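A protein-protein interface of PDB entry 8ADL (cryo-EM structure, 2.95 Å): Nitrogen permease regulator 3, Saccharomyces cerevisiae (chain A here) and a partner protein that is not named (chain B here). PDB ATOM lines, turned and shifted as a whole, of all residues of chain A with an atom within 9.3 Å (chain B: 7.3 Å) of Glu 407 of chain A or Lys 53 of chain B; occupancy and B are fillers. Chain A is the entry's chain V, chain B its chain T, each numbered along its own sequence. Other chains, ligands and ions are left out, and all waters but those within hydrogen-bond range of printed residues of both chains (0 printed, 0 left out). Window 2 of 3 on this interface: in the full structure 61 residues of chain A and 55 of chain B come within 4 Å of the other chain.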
ATOM      1  N   VAL A  16      35.642 -32.711   7.371  1.00  0.00           N
ATOM      2  CA  VAL A  16      34.214 -32.978   7.275  1.00  0.00           C
ATOM      3  C   VAL A  16      34.029 -34.398   6.766  1.00  0.00           C
ATOM      4  O   VAL A  16      34.399 -34.716   5.629  1.00  0.00           O
ATOM      5  CB  VAL A  16      33.517 -31.965   6.354  1.00  0.00           C
ATOM      6  CG1 VAL A  16      32.069 -32.368   6.112  1.00  0.00           C
ATOM      7  CG2 VAL A  16      33.603 -30.564   6.943  1.00  0.00           C
ATOM      8  N   ILE A  17      33.460 -35.251   7.611  1.00  0.00           N
ATOM      9  CA  ILE A  17      33.174 -36.631   7.261  1.00  0.00           C
ATOM     10  C   ILE A  17      31.663 -36.813   7.219  1.00  0.00           C
ATOM     11  O   ILE A  17      30.894 -36.016   7.763  1.00  0.00           O
ATOM     12  CB  ILE A  17      33.829 -37.634   8.236  1.00  0.00           C
ATOM     13  CG1 ILE A  17      33.075 -37.674   9.567  1.00  0.00           C
ATOM     14  CG2 ILE A  17      35.293 -37.282   8.465  1.00  0.00           C
ATOM     15  CD1 ILE A  17      33.205 -38.990  10.298  1.00  0.00           C
ATOM     16  N   SER A  18      31.235 -37.876   6.545  1.00  0.00           N
ATOM     17  CA  SER A  18      29.822 -38.193   6.418  1.00  0.00           C
ATOM     18  C   SER A  18      29.613 -39.670   6.714  1.00  0.00           C
ATOM     19  O   SER A  18      30.472 -40.506   6.423  1.00  0.00           O
ATOM     20  CB  SER A  18      29.296 -37.857   5.016  1.00  0.00           C
ATOM     21  OG  SER A  18      27.907 -38.118   4.917  1.00  0.00           O
ATOM     22  N   GLY A  22      24.374 -39.139   8.781  1.00  0.00           N
ATOM     23  CA  GLY A  22      24.448 -37.780   8.305  1.00  0.00           C
ATOM     24  C   GLY A  22      25.842 -37.204   8.460  1.00  0.00           C
ATOM     25  O   GLY A  22      26.684 -37.742   9.184  1.00  0.00           O
ATOM     26  N   PRO A  23      26.113 -36.096   7.773  1.00  0.00           N
ATOM     27  CA  PRO A  23      27.444 -35.490   7.856  1.00  0.00           C
ATOM     28  C   PRO A  23      27.662 -34.773   9.179  1.00  0.00           C
ATOM     29  O   PRO A  23      26.724 -34.289   9.819  1.00  0.00           O
ATOM     30  CB  PRO A  23      27.456 -34.505   6.684  1.00  0.00           C
ATOM     31  CG  PRO A  23      26.024 -34.119   6.521  1.00  0.00           C
ATOM     32  CD  PRO A  23      25.208 -35.330   6.897  1.00  0.00           C
ATOM     33  N   GLN A  24      28.928 -34.711   9.585  1.00  0.00           N
ATOM     34  CA  GLN A  24      29.325 -34.033  10.809  1.00  0.00           C
ATOM     35  C   GLN A  24      30.707 -33.427  10.595  1.00  0.00           C
ATOM     36  O   GLN A  24      31.271 -33.490   9.498  1.00  0.00           O
ATOM     37  CB  GLN A  24      29.318 -34.996  12.001  1.00  0.00           C
ATOM     38  CG  GLN A  24      30.345 -36.113  11.898  1.00  0.00           C
ATOM     39  CD  GLN A  24      30.274 -37.083  13.061  1.00  0.00           C
ATOM     40  OE1 GLN A  24      31.002 -38.074  13.104  1.00  0.00           O
ATOM     41  NE2 GLN A  24      29.388 -36.804  14.010  1.00  0.00           N
ATOM     42  N   ILE A  25      31.253 -32.834  11.653  1.00  0.00           N
ATOM     43  CA  ILE A  25      32.601 -32.285  11.622  1.00  0.00           C
ATOM     44  C   ILE A  25      33.412 -32.954  12.722  1.00  0.00           C
ATOM     45  O   ILE A  25      32.864 -33.454  13.711  1.00  0.00           O
ATOM     46  CB  ILE A  25      32.599 -30.742  11.761  1.00  0.00           C
ATOM     47  CG1 ILE A  25      33.854 -30.138  11.123  1.00  0.00           C
ATOM     48  CG2 ILE A  25      32.475 -30.306  13.216  1.00  0.00           C
ATOM     49  CD1 ILE A  25      33.689 -28.699  10.704  1.00  0.00           C
ATOM     50  N   PHE A 400      29.079 -19.455  10.580  1.00  0.00           N
ATOM     51  CA  PHE A 400      28.317 -20.643  10.223  1.00  0.00           C
ATOM     52  C   PHE A 400      28.485 -21.681  11.321  1.00  0.00           C
ATOM     53  O   PHE A 400      29.538 -21.768  11.955  1.00  0.00           O
ATOM     54  CB  PHE A 400      28.774 -21.242   8.879  1.00  0.00           C
ATOM     55  CG  PHE A 400      28.760 -20.268   7.734  1.00  0.00           C
ATOM     56  CD1 PHE A 400      27.616 -19.553   7.423  1.00  0.00           C
ATOM     57  CD2 PHE A 400      29.897 -20.067   6.969  1.00  0.00           C
ATOM     58  CE1 PHE A 400      27.601 -18.658   6.370  1.00  0.00           C
ATOM     59  CE2 PHE A 400      29.891 -19.171   5.915  1.00  0.00           C
ATOM     60  CZ  PHE A 400      28.739 -18.466   5.617  1.00  0.00           C
ATOM     61  N   ASP A 401      27.448 -22.490  11.520  1.00  0.00           N
ATOM     62  CA  ASP A 401      27.500 -23.580  12.483  1.00  0.00           C
ATOM     63  C   ASP A 401      28.323 -24.749  11.946  1.00  0.00           C
ATOM     64  O   ASP A 401      28.620 -24.834  10.751  1.00  0.00           O
ATOM     65  CB  ASP A 401      26.089 -24.052  12.830  1.00  0.00           C
ATOM     66  CG  ASP A 401      25.263 -22.969  13.498  1.00  0.00           C
ATOM     67  OD1 ASP A 401      25.854 -22.092  14.162  1.00  0.00           O
ATOM     68  OD2 ASP A 401      24.022 -22.996  13.358  1.00  0.00           O
ATOM     69  N   ASN A 402      28.709 -25.650  12.859  1.00  0.00           N
ATOM     70  CA  ASN A 402      29.404 -26.868  12.449  1.00  0.00           C
ATOM     71  C   ASN A 402      28.499 -27.752  11.601  1.00  0.00           C
ATOM     72  O   ASN A 402      28.937 -28.312  10.588  1.00  0.00           O
ATOM     73  CB  ASN A 402      29.903 -27.645  13.667  1.00  0.00           C
ATOM     74  CG  ASN A 402      31.217 -27.117  14.201  1.00  0.00           C
ATOM     75  OD1 ASN A 402      32.046 -26.610  13.448  1.00  0.00           O
ATOM     76  ND2 ASN A 402      31.433 -27.275  15.500  1.00  0.00           N
ATOM     77  N   ASP A 403      27.235 -27.895  12.009  1.00  0.00           N
ATOM     78  CA  ASP A 403      26.284 -28.691  11.240  1.00  0.00           C
ATOM     79  C   ASP A 403      25.986 -28.034   9.901  1.00  0.00           C
ATOM     80  O   ASP A 403      25.805 -28.729   8.897  1.00  0.00           O
ATOM     81  CB  ASP A 403      24.996 -28.894  12.038  1.00  0.00           C
ATOM     82  CG  ASP A 403      25.187 -29.817  13.226  1.00  0.00           C
ATOM     83  OD1 ASP A 403      26.241 -30.484  13.300  1.00  0.00           O
ATOM     84  OD2 ASP A 403      24.283 -29.875  14.086  1.00  0.00           O
ATOM     85  N   PHE A 404      25.965 -26.700   9.868  1.00  0.00           N
ATOM     86  CA  PHE A 404      25.750 -25.969   8.624  1.00  0.00           C
ATOM     87  C   PHE A 404      26.897 -26.201   7.645  1.00  0.00           C
ATOM     88  O   PHE A 404      26.668 -26.508   6.465  1.00  0.00           O
ATOM     89  CB  PHE A 404      25.596 -24.481   8.936  1.00  0.00           C
ATOM     90  CG  PHE A 404      24.980 -23.690   7.828  1.00  0.00           C
ATOM     91  CD1 PHE A 404      23.661 -23.896   7.467  1.00  0.00           C
ATOM     92  CD2 PHE A 404      25.717 -22.730   7.152  1.00  0.00           C
ATOM     93  CE1 PHE A 404      23.087 -23.168   6.450  1.00  0.00           C
ATOM     94  CE2 PHE A 404      25.147 -21.996   6.134  1.00  0.00           C
ATOM     95  CZ  PHE A 404      23.828 -22.216   5.782  1.00  0.00           C
ATOM     96  N   VAL A 405      28.140 -26.065   8.127  1.00  0.00           N
ATOM     97  CA  VAL A 405      29.319 -26.289   7.292  1.00  0.00           C
ATOM     98  C   VAL A 405      29.369 -27.735   6.816  1.00  0.00           C
ATOM     99  O   VAL A 405      29.610 -28.004   5.634  1.00  0.00           O
ATOM    100  CB  VAL A 405      30.599 -25.890   8.054  1.00  0.00           C
ATOM    101  CG1 VAL A 405      31.845 -26.402   7.345  1.00  0.00           C
ATOM    102  CG2 VAL A 405      30.675 -24.382   8.200  1.00  0.00           C
ATOM    103  N   ALA A 406      29.094 -28.686   7.714  1.00  0.00           N
ATOM    104  CA  ALA A 406      29.018 -30.088   7.322  1.00  0.00           C
ATOM    105  C   ALA A 406      27.861 -30.367   6.369  1.00  0.00           C
ATOM    106  O   ALA A 406      27.889 -31.377   5.660  1.00  0.00           O
ATOM    107  CB  ALA A 406      28.894 -30.978   8.560  1.00  0.00           C
ATOM    108  N   GLU A 407      26.847 -29.500   6.337  1.00  0.00           N
ATOM    109  CA  GLU A 407      25.778 -29.645   5.358  1.00  0.00           C
ATOM    110  C   GLU A 407      26.214 -29.177   3.974  1.00  0.00           C
ATOM    111  O   GLU A 407      26.041 -29.904   2.990  1.00  0.00           O
ATOM    112  CB  GLU A 407      24.532 -28.883   5.812  1.00  0.00           C
ATOM    113  CG  GLU A 407      23.389 -28.931   4.810  1.00  0.00           C
ATOM    114  CD  GLU A 407      22.049 -28.607   5.436  1.00  0.00           C
ATOM    115  OE1 GLU A 407      22.030 -27.939   6.490  1.00  0.00           O
ATOM    116  OE2 GLU A 407      21.014 -29.022   4.873  1.00  0.00           O
ATOM    117  N   PHE A 408      26.778 -27.970   3.862  1.00  0.00           N
ATOM    118  CA  PHE A 408      27.074 -27.479   2.517  1.00  0.00           C
ATOM    119  C   PHE A 408      28.477 -27.836   2.026  1.00  0.00           C
ATOM    120  O   PHE A 408      28.814 -27.500   0.885  1.00  0.00           O
ATOM    121  CB  PHE A 408      26.810 -25.954   2.408  1.00  0.00           C
ATOM    122  CG  PHE A 408      27.856 -25.052   3.051  1.00  0.00           C
ATOM    123  CD1 PHE A 408      28.994 -24.648   2.357  1.00  0.00           C
ATOM    124  CD2 PHE A 408      27.647 -24.534   4.317  1.00  0.00           C
ATOM    125  CE1 PHE A 408      29.927 -23.808   2.945  1.00  0.00           C
ATOM    126  CE2 PHE A 408      28.574 -23.690   4.908  1.00  0.00           C
ATOM    127  CZ  PHE A 408      29.713 -23.328   4.222  1.00  0.00           C
ATOM    128  N   CYS A 409      29.299 -28.507   2.834  1.00  0.00           N
ATOM    129  CA  CYS A 409      30.582 -29.027   2.373  1.00  0.00           C
ATOM    130  C   CYS A 409      30.584 -30.541   2.195  1.00  0.00           C
ATOM    131  O   CYS A 409      31.651 -31.127   1.989  1.00  0.00           O
ATOM    132  CB  CYS A 409      31.711 -28.615   3.321  1.00  0.00           C
ATOM    133  SG  CYS A 409      31.947 -26.829   3.469  1.00  0.00           S
ATOM    134  N   SER A 410      29.421 -31.192   2.270  1.00  0.00           N
ATOM    135  CA  SER A 410      29.295 -32.626   2.014  1.00  0.00           C
ATOM    136  C   SER A 410      28.330 -32.841   0.853  1.00  0.00           C
ATOM    137  O   SER A 410      27.130 -33.079   1.062  1.00  0.00           O
ATOM    138  CB  SER A 410      28.827 -33.379   3.258  1.00  0.00           C
ATOM    139  OG  SER A 410      27.455 -33.134   3.515  1.00  0.00           O
ATOM    140  N   PRO A 411      28.814 -32.762  -0.379  1.00  0.00           N
ATOM    141  CA  PRO A 411      27.934 -32.818  -1.547  1.00  0.00           C
ATOM    142  C   PRO A 411      27.564 -34.259  -1.888  1.00  0.00           C
ATOM    143  O   PRO A 411      27.942 -35.210  -1.206  1.00  0.00           O
ATOM    144  CB  PRO A 411      28.779 -32.174  -2.645  1.00  0.00           C
ATOM    145  CG  PRO A 411      30.181 -32.500  -2.265  1.00  0.00           C
ATOM    146  CD  PRO A 411      30.226 -32.570  -0.760  1.00  0.00           C
ATOM    147  N   GLU A 412      26.808 -34.401  -2.973  1.00  0.00           N
ATOM    148  CA  GLU A 412      26.344 -35.700  -3.440  1.00  0.00           C
ATOM    149  C   GLU A 412      27.484 -36.476  -4.102  1.00  0.00           C
ATOM    150  O   GLU A 412      28.613 -35.993  -4.246  1.00  0.00           O
ATOM    151  CB  GLU A 412      25.168 -35.526  -4.397  1.00  0.00           C
ATOM    152  CG  GLU A 412      23.810 -35.527  -3.713  1.00  0.00           C
ATOM    153  CD  GLU A 412      23.454 -34.181  -3.114  1.00  0.00           C
ATOM    154  OE1 GLU A 412      24.122 -33.181  -3.452  1.00  0.00           O
ATOM    155  OE2 GLU A 412      22.505 -34.124  -2.304  1.00  0.00           O
ATOM    156  N   PHE A 420      35.990 -29.494  -5.607  1.00  0.00           N
ATOM    157  CA  PHE A 420      34.911 -28.786  -4.917  1.00  0.00           C
ATOM    158  C   PHE A 420      35.328 -27.328  -4.760  1.00  0.00           C
ATOM    159  O   PHE A 420      36.054 -26.976  -3.828  1.00  0.00           O
ATOM    160  CB  PHE A 420      34.610 -29.439  -3.573  1.00  0.00           C
ATOM    161  CG  PHE A 420      33.485 -28.791  -2.818  1.00  0.00           C
ATOM    162  CD1 PHE A 420      32.167 -29.043  -3.165  1.00  0.00           C
ATOM    163  CD2 PHE A 420      33.743 -27.943  -1.752  1.00  0.00           C
ATOM    164  CE1 PHE A 420      31.127 -28.453  -2.472  1.00  0.00           C
ATOM    165  CE2 PHE A 420      32.707 -27.350  -1.053  1.00  0.00           C
ATOM    166  CZ  PHE A 420      31.398 -27.604  -1.413  1.00  0.00           C
ATOM    167  N   PHE A 422      33.694 -23.566  -4.165  1.00  0.00           N
ATOM    168  CA  PHE A 422      32.463 -22.986  -3.636  1.00  0.00           C
ATOM    169  C   PHE A 422      32.804 -21.673  -2.950  1.00  0.00           C
ATOM    170  O   PHE A 422      33.549 -21.670  -1.966  1.00  0.00           O
ATOM    171  CB  PHE A 422      31.790 -23.953  -2.657  1.00  0.00           C
ATOM    172  CG  PHE A 422      30.383 -23.575  -2.295  1.00  0.00           C
ATOM    173  CD1 PHE A 422      29.331 -23.876  -3.144  1.00  0.00           C
ATOM    174  CD2 PHE A 422      30.110 -22.922  -1.103  1.00  0.00           C
ATOM    175  CE1 PHE A 422      28.032 -23.531  -2.816  1.00  0.00           C
ATOM    176  CE2 PHE A 422      28.814 -22.574  -0.767  1.00  0.00           C
ATOM    177  CZ  PHE A 422      27.774 -22.879  -1.625  1.00  0.00           C
ATOM    178  N   MET A 532      32.511 -40.905   3.188  1.00  0.00           N
ATOM    179  CA  MET A 532      33.048 -39.678   2.619  1.00  0.00           C
ATOM    180  C   MET A 532      33.816 -38.946   3.708  1.00  0.00           C
ATOM    181  O   MET A 532      33.377 -38.905   4.859  1.00  0.00           O
ATOM    182  CB  MET A 532      31.935 -38.784   2.053  1.00  0.00           C
ATOM    183  CG  MET A 532      32.381 -37.817   0.957  1.00  0.00           C
ATOM    184  SD  MET A 532      33.119 -36.291   1.572  1.00  0.00           S
ATOM    185  CE  MET A 532      31.856 -35.741   2.715  1.00  0.00           C
ATOM    186  N   HIS A 534      36.214 -35.082   3.897  1.00  0.00           N
ATOM    187  CA  HIS A 534      36.544 -33.866   3.155  1.00  0.00           C
ATOM    188  C   HIS A 534      37.445 -32.982   4.005  1.00  0.00           C
ATOM    189  O   HIS A 534      37.015 -32.462   5.040  1.00  0.00           O
ATOM    190  CB  HIS A 534      35.280 -33.109   2.746  1.00  0.00           C
ATOM    191  CG  HIS A 534      35.538 -31.952   1.832  1.00  0.00           C
ATOM    192  ND1 HIS A 534      34.712 -30.850   1.774  1.00  0.00           N
ATOM    193  CD2 HIS A 534      36.541 -31.716   0.953  1.00  0.00           C
ATOM    194  CE1 HIS A 534      35.187 -29.991   0.891  1.00  0.00           C
ATOM    195  NE2 HIS A 534      36.296 -30.492   0.378  1.00  0.00           N
ATOM    196  N   ASN B  48      20.327 -27.873  -3.506  1.00  0.00           N
ATOM    197  CA  ASN B  48      20.453 -27.389  -2.140  1.00  0.00           C
ATOM    198  C   ASN B  48      21.442 -26.239  -2.026  1.00  0.00           C
ATOM    199  O   ASN B  48      21.564 -25.648  -0.949  1.00  0.00           O
ATOM    200  CB  ASN B  48      20.882 -28.528  -1.209  1.00  0.00           C
ATOM    201  CG  ASN B  48      19.728 -29.433  -0.826  1.00  0.00           C
ATOM    202  OD1 ASN B  48      18.624 -28.965  -0.547  1.00  0.00           O
ATOM    203  ND2 ASN B  48      19.978 -30.737  -0.810  1.00  0.00           N
ATOM    204  N   TYR B  49      22.152 -25.919  -3.108  1.00  0.00           N
ATOM    205  CA  TYR B  49      22.974 -24.720  -3.181  1.00  0.00           C
ATOM    206  C   TYR B  49      22.270 -23.568  -3.880  1.00  0.00           C
ATOM    207  O   TYR B  49      22.534 -22.405  -3.557  1.00  0.00           O
ATOM    208  CB  TYR B  49      24.270 -25.037  -3.934  1.00  0.00           C
ATOM    209  CG  TYR B  49      25.079 -26.154  -3.312  1.00  0.00           C
ATOM    210  CD1 TYR B  49      25.196 -26.276  -1.932  1.00  0.00           C
ATOM    211  CD2 TYR B  49      25.690 -27.114  -4.110  1.00  0.00           C
ATOM    212  CE1 TYR B  49      25.923 -27.311  -1.366  1.00  0.00           C
ATOM    213  CE2 TYR B  49      26.417 -28.150  -3.555  1.00  0.00           C
ATOM    214  CZ  TYR B  49      26.531 -28.245  -2.184  1.00  0.00           C
ATOM    215  OH  TYR B  49      27.256 -29.276  -1.632  1.00  0.00           O
ATOM    216  N   ILE B  51      18.891 -23.060  -3.815  1.00  0.00           N
ATOM    217  CA  ILE B  51      17.991 -22.605  -2.761  1.00  0.00           C
ATOM    218  C   ILE B  51      18.506 -23.148  -1.434  1.00  0.00           C
ATOM    219  O   ILE B  51      18.019 -24.180  -0.949  1.00  0.00           O
ATOM    220  CB  ILE B  51      16.542 -23.044  -3.028  1.00  0.00           C
ATOM    221  CG1 ILE B  51      16.163 -22.784  -4.489  1.00  0.00           C
ATOM    222  CG2 ILE B  51      15.580 -22.311  -2.097  1.00  0.00           C
ATOM    223  CD1 ILE B  51      16.062 -21.316  -4.849  1.00  0.00           C
ATOM    224  N   PRO B  52      19.500 -22.502  -0.825  1.00  0.00           N
ATOM    225  CA  PRO B  52      20.051 -23.004   0.436  1.00  0.00           C
ATOM    226  C   PRO B  52      19.256 -22.485   1.619  1.00  0.00           C
ATOM    227  O   PRO B  52      18.195 -21.878   1.443  1.00  0.00           O
ATOM    228  CB  PRO B  52      21.482 -22.457   0.430  1.00  0.00           C
ATOM    229  CG  PRO B  52      21.388 -21.179  -0.368  1.00  0.00           C
ATOM    230  CD  PRO B  52      20.135 -21.234  -1.223  1.00  0.00           C
ATOM    231  N   LYS B  53      19.750 -22.739   2.828  1.00  0.00           N
ATOM    232  CA  LYS B  53      19.159 -22.152   4.014  1.00  0.00           C
ATOM    233  C   LYS B  53      19.362 -20.634   4.000  1.00  0.00           C
ATOM    234  O   LYS B  53      20.280 -20.132   3.346  1.00  0.00           O
ATOM    235  CB  LYS B  53      19.784 -22.776   5.261  1.00  0.00           C
ATOM    236  CG  LYS B  53      19.547 -24.274   5.381  1.00  0.00           C
ATOM    237  CD  LYS B  53      19.770 -24.759   6.803  1.00  0.00           C
ATOM    238  CE  LYS B  53      19.239 -26.172   6.991  1.00  0.00           C
ATOM    239  NZ  LYS B  53      17.778 -26.257   6.717  1.00  0.00           N
ATOM    240  N   PRO B  54      18.506 -19.879   4.705  1.00  0.00           N
ATOM    241  CA  PRO B  54      18.600 -18.405   4.660  1.00  0.00           C
ATOM    242  C   PRO B  54      19.897 -17.813   5.207  1.00  0.00           C
ATOM    243  O   PRO B  54      20.121 -16.610   5.018  1.00  0.00           O
ATOM    244  CB  PRO B  54      17.398 -17.952   5.501  1.00  0.00           C
ATOM    245  CG  PRO B  54      16.418 -19.051   5.355  1.00  0.00           C
ATOM    246  CD  PRO B  54      17.229 -20.314   5.305  1.00  0.00           C
ATOM    247  N   ILE B  55      20.741 -18.596   5.881  1.00  0.00           N
ATOM    248  CA  ILE B  55      22.059 -18.102   6.269  1.00  0.00           C
ATOM    249  C   ILE B  55      22.923 -17.887   5.029  1.00  0.00           C
ATOM    250  O   ILE B  55      23.571 -16.845   4.877  1.00  0.00           O
ATOM    251  CB  ILE B  55      22.732 -19.058   7.276  1.00  0.00           C
ATOM    252  CG1 ILE B  55      21.953 -19.141   8.599  1.00  0.00           C
ATOM    253  CG2 ILE B  55      24.153 -18.617   7.565  1.00  0.00           C
ATOM    254  CD1 ILE B  55      20.912 -20.253   8.685  1.00  0.00           C
ATOM    255  N   LEU B  56      22.921 -18.858   4.111  1.00  0.00           N
ATOM    256  CA  LEU B  56      23.680 -18.746   2.870  1.00  0.00           C
ATOM    257  C   LEU B  56      23.006 -17.847   1.841  1.00  0.00           C
ATOM    258  O   LEU B  56      23.644 -17.483   0.848  1.00  0.00           O
ATOM    259  CB  LEU B  56      23.909 -20.131   2.256  1.00  0.00           C
ATOM    260  CG  LEU B  56      25.159 -20.894   2.701  1.00  0.00           C
ATOM    261  CD1 LEU B  56      25.392 -22.113   1.817  1.00  0.00           C
ATOM    262  CD2 LEU B  56      26.384 -19.988   2.717  1.00  0.00           C
ATOM    263  N   CYS B  57      21.743 -17.490   2.052  1.00  0.00           N
ATOM    264  CA  CYS B  57      21.009 -16.662   1.110  1.00  0.00           C
ATOM    265  C   CYS B  57      21.483 -15.213   1.192  1.00  0.00           C
ATOM    266  O   CYS B  57      22.130 -14.799   2.160  1.00  0.00           O
ATOM    267  CB  CYS B  57      19.507 -16.742   1.377  1.00  0.00           C
ATOM    268  SG  CYS B  57      18.687 -18.160   0.613  1.00  0.00           S
ATOM    269  N   HIS B  58      21.157 -14.450   0.138  1.00  0.00           N
ATOM    270  CA  HIS B  58      21.627 -13.074  -0.071  1.00  0.00           C
ATOM    271  C   HIS B  58      23.153 -12.990  -0.060  1.00  0.00           C
ATOM    272  O   HIS B  58      23.740 -12.045   0.471  1.00  0.00           O
ATOM    273  CB  HIS B  58      21.020 -12.112   0.953  1.00  0.00           C
ATOM    274  CG  HIS B  58      19.560 -12.331   1.192  1.00  0.00           C
ATOM    275  ND1 HIS B  58      19.026 -12.460   2.456  1.00  0.00           N
ATOM    276  CD2 HIS B  58      18.522 -12.450   0.331  1.00  0.00           C
ATOM    277  CE1 HIS B  58      17.722 -12.647   2.364  1.00  0.00           C
ATOM    278  NE2 HIS B  58      17.390 -12.644   1.085  1.00  0.00           N
ATOM    279  N   PRO B  74      21.237 -16.383  -4.425  1.00  0.00           N
ATOM    280  CA  PRO B  74      19.957 -16.820  -3.847  1.00  0.00           C
ATOM    281  C   PRO B  74      19.330 -15.741  -2.977  1.00  0.00           C
ATOM    282  O   PRO B  74      20.006 -15.077  -2.188  1.00  0.00           O
ATOM    283  CB  PRO B  74      20.343 -18.049  -3.016  1.00  0.00           C
ATOM    284  CG  PRO B  74      21.803 -17.885  -2.748  1.00  0.00           C
ATOM    285  CD  PRO B  74      22.361 -17.214  -3.965  1.00  0.00           C
ATOM    286  N   THR B  76      15.929 -14.983  -0.421  1.00  0.00           N
ATOM    287  CA  THR B  76      14.809 -15.491   0.359  1.00  0.00           C
ATOM    288  C   THR B  76      14.131 -14.320   1.052  1.00  0.00           C
ATOM    289  O   THR B  76      14.784 -13.560   1.773  1.00  0.00           O
ATOM    290  CB  THR B  76      15.277 -16.528   1.390  1.00  0.00           C
ATOM    291  OG1 THR B  76      15.693 -17.721   0.714  1.00  0.00           O
ATOM    292  CG2 THR B  76      14.157 -16.870   2.362  1.00  0.00           C
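OH of Tyr 49 of chain B is in hydrogen-bond range of O of Phe 408 of chain A.
Printed residues of chain A that touch a printed residue of chain B: Phe 400, Phe 404, Glu 407, Phe 408, Pro 411 and Phe 422.
Along chain B the printed residues that touch a printed residue of chain A span positions 49 to 56.
Among the printed residues, no Asp or Glu carboxylate lies within 4 Å of a Lys or Arg side-chain nitrogen of the other chain.
Of chain B, only Lys 53 (3.3 Å) comes within 4 Å of Glu 407 of chain A.
Lys 53 of chain B touches just these residues of chain A: Phe 404 and Glu 407.
No residue of chain A comes within 4 Å of Pro 52 of chain B.
No residue of chain A comes within 4 Å of Pro 54 of chain B.
Printed residues of chain A within 4 Å of Ile 55 of chain B: Phe 400 (3.6 Å) and Phe 404 (3.7 Å).
Of the printed residues of chain A, Leu 56 of chain B touches Phe 404.
Of the printed residues of chain B, Phe 408 of chain A touches Tyr 49.
Asp 401 of chain A touches none of the printed residues of chain B.
The nearest residue of chain A that does not touch Lys 53 of chain B is Asp 403 of chain A (7.3 Å).
The backbone carbonyl oxygen of Lys 53 of chain B is in hydrogen-bond range of the side-chain sulfur of Cys 57 of chain B (3.7 Å).
Among the printed residues, merely in contact across the chains: Phe 400 of chain A with Ile 55 of chain B, Phe 404 of chain A with Lys 53 of chain B, Phe 404 of chain A with Ile 55 of chain B, Phe 404 of chain A with Leu 56 of chain B, Glu 407 of chain A with Lys 53 of chain B, Pro 411 of chain A with Tyr 49 of chain B and Phe 422 of chain A with Tyr 49 of chain B.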
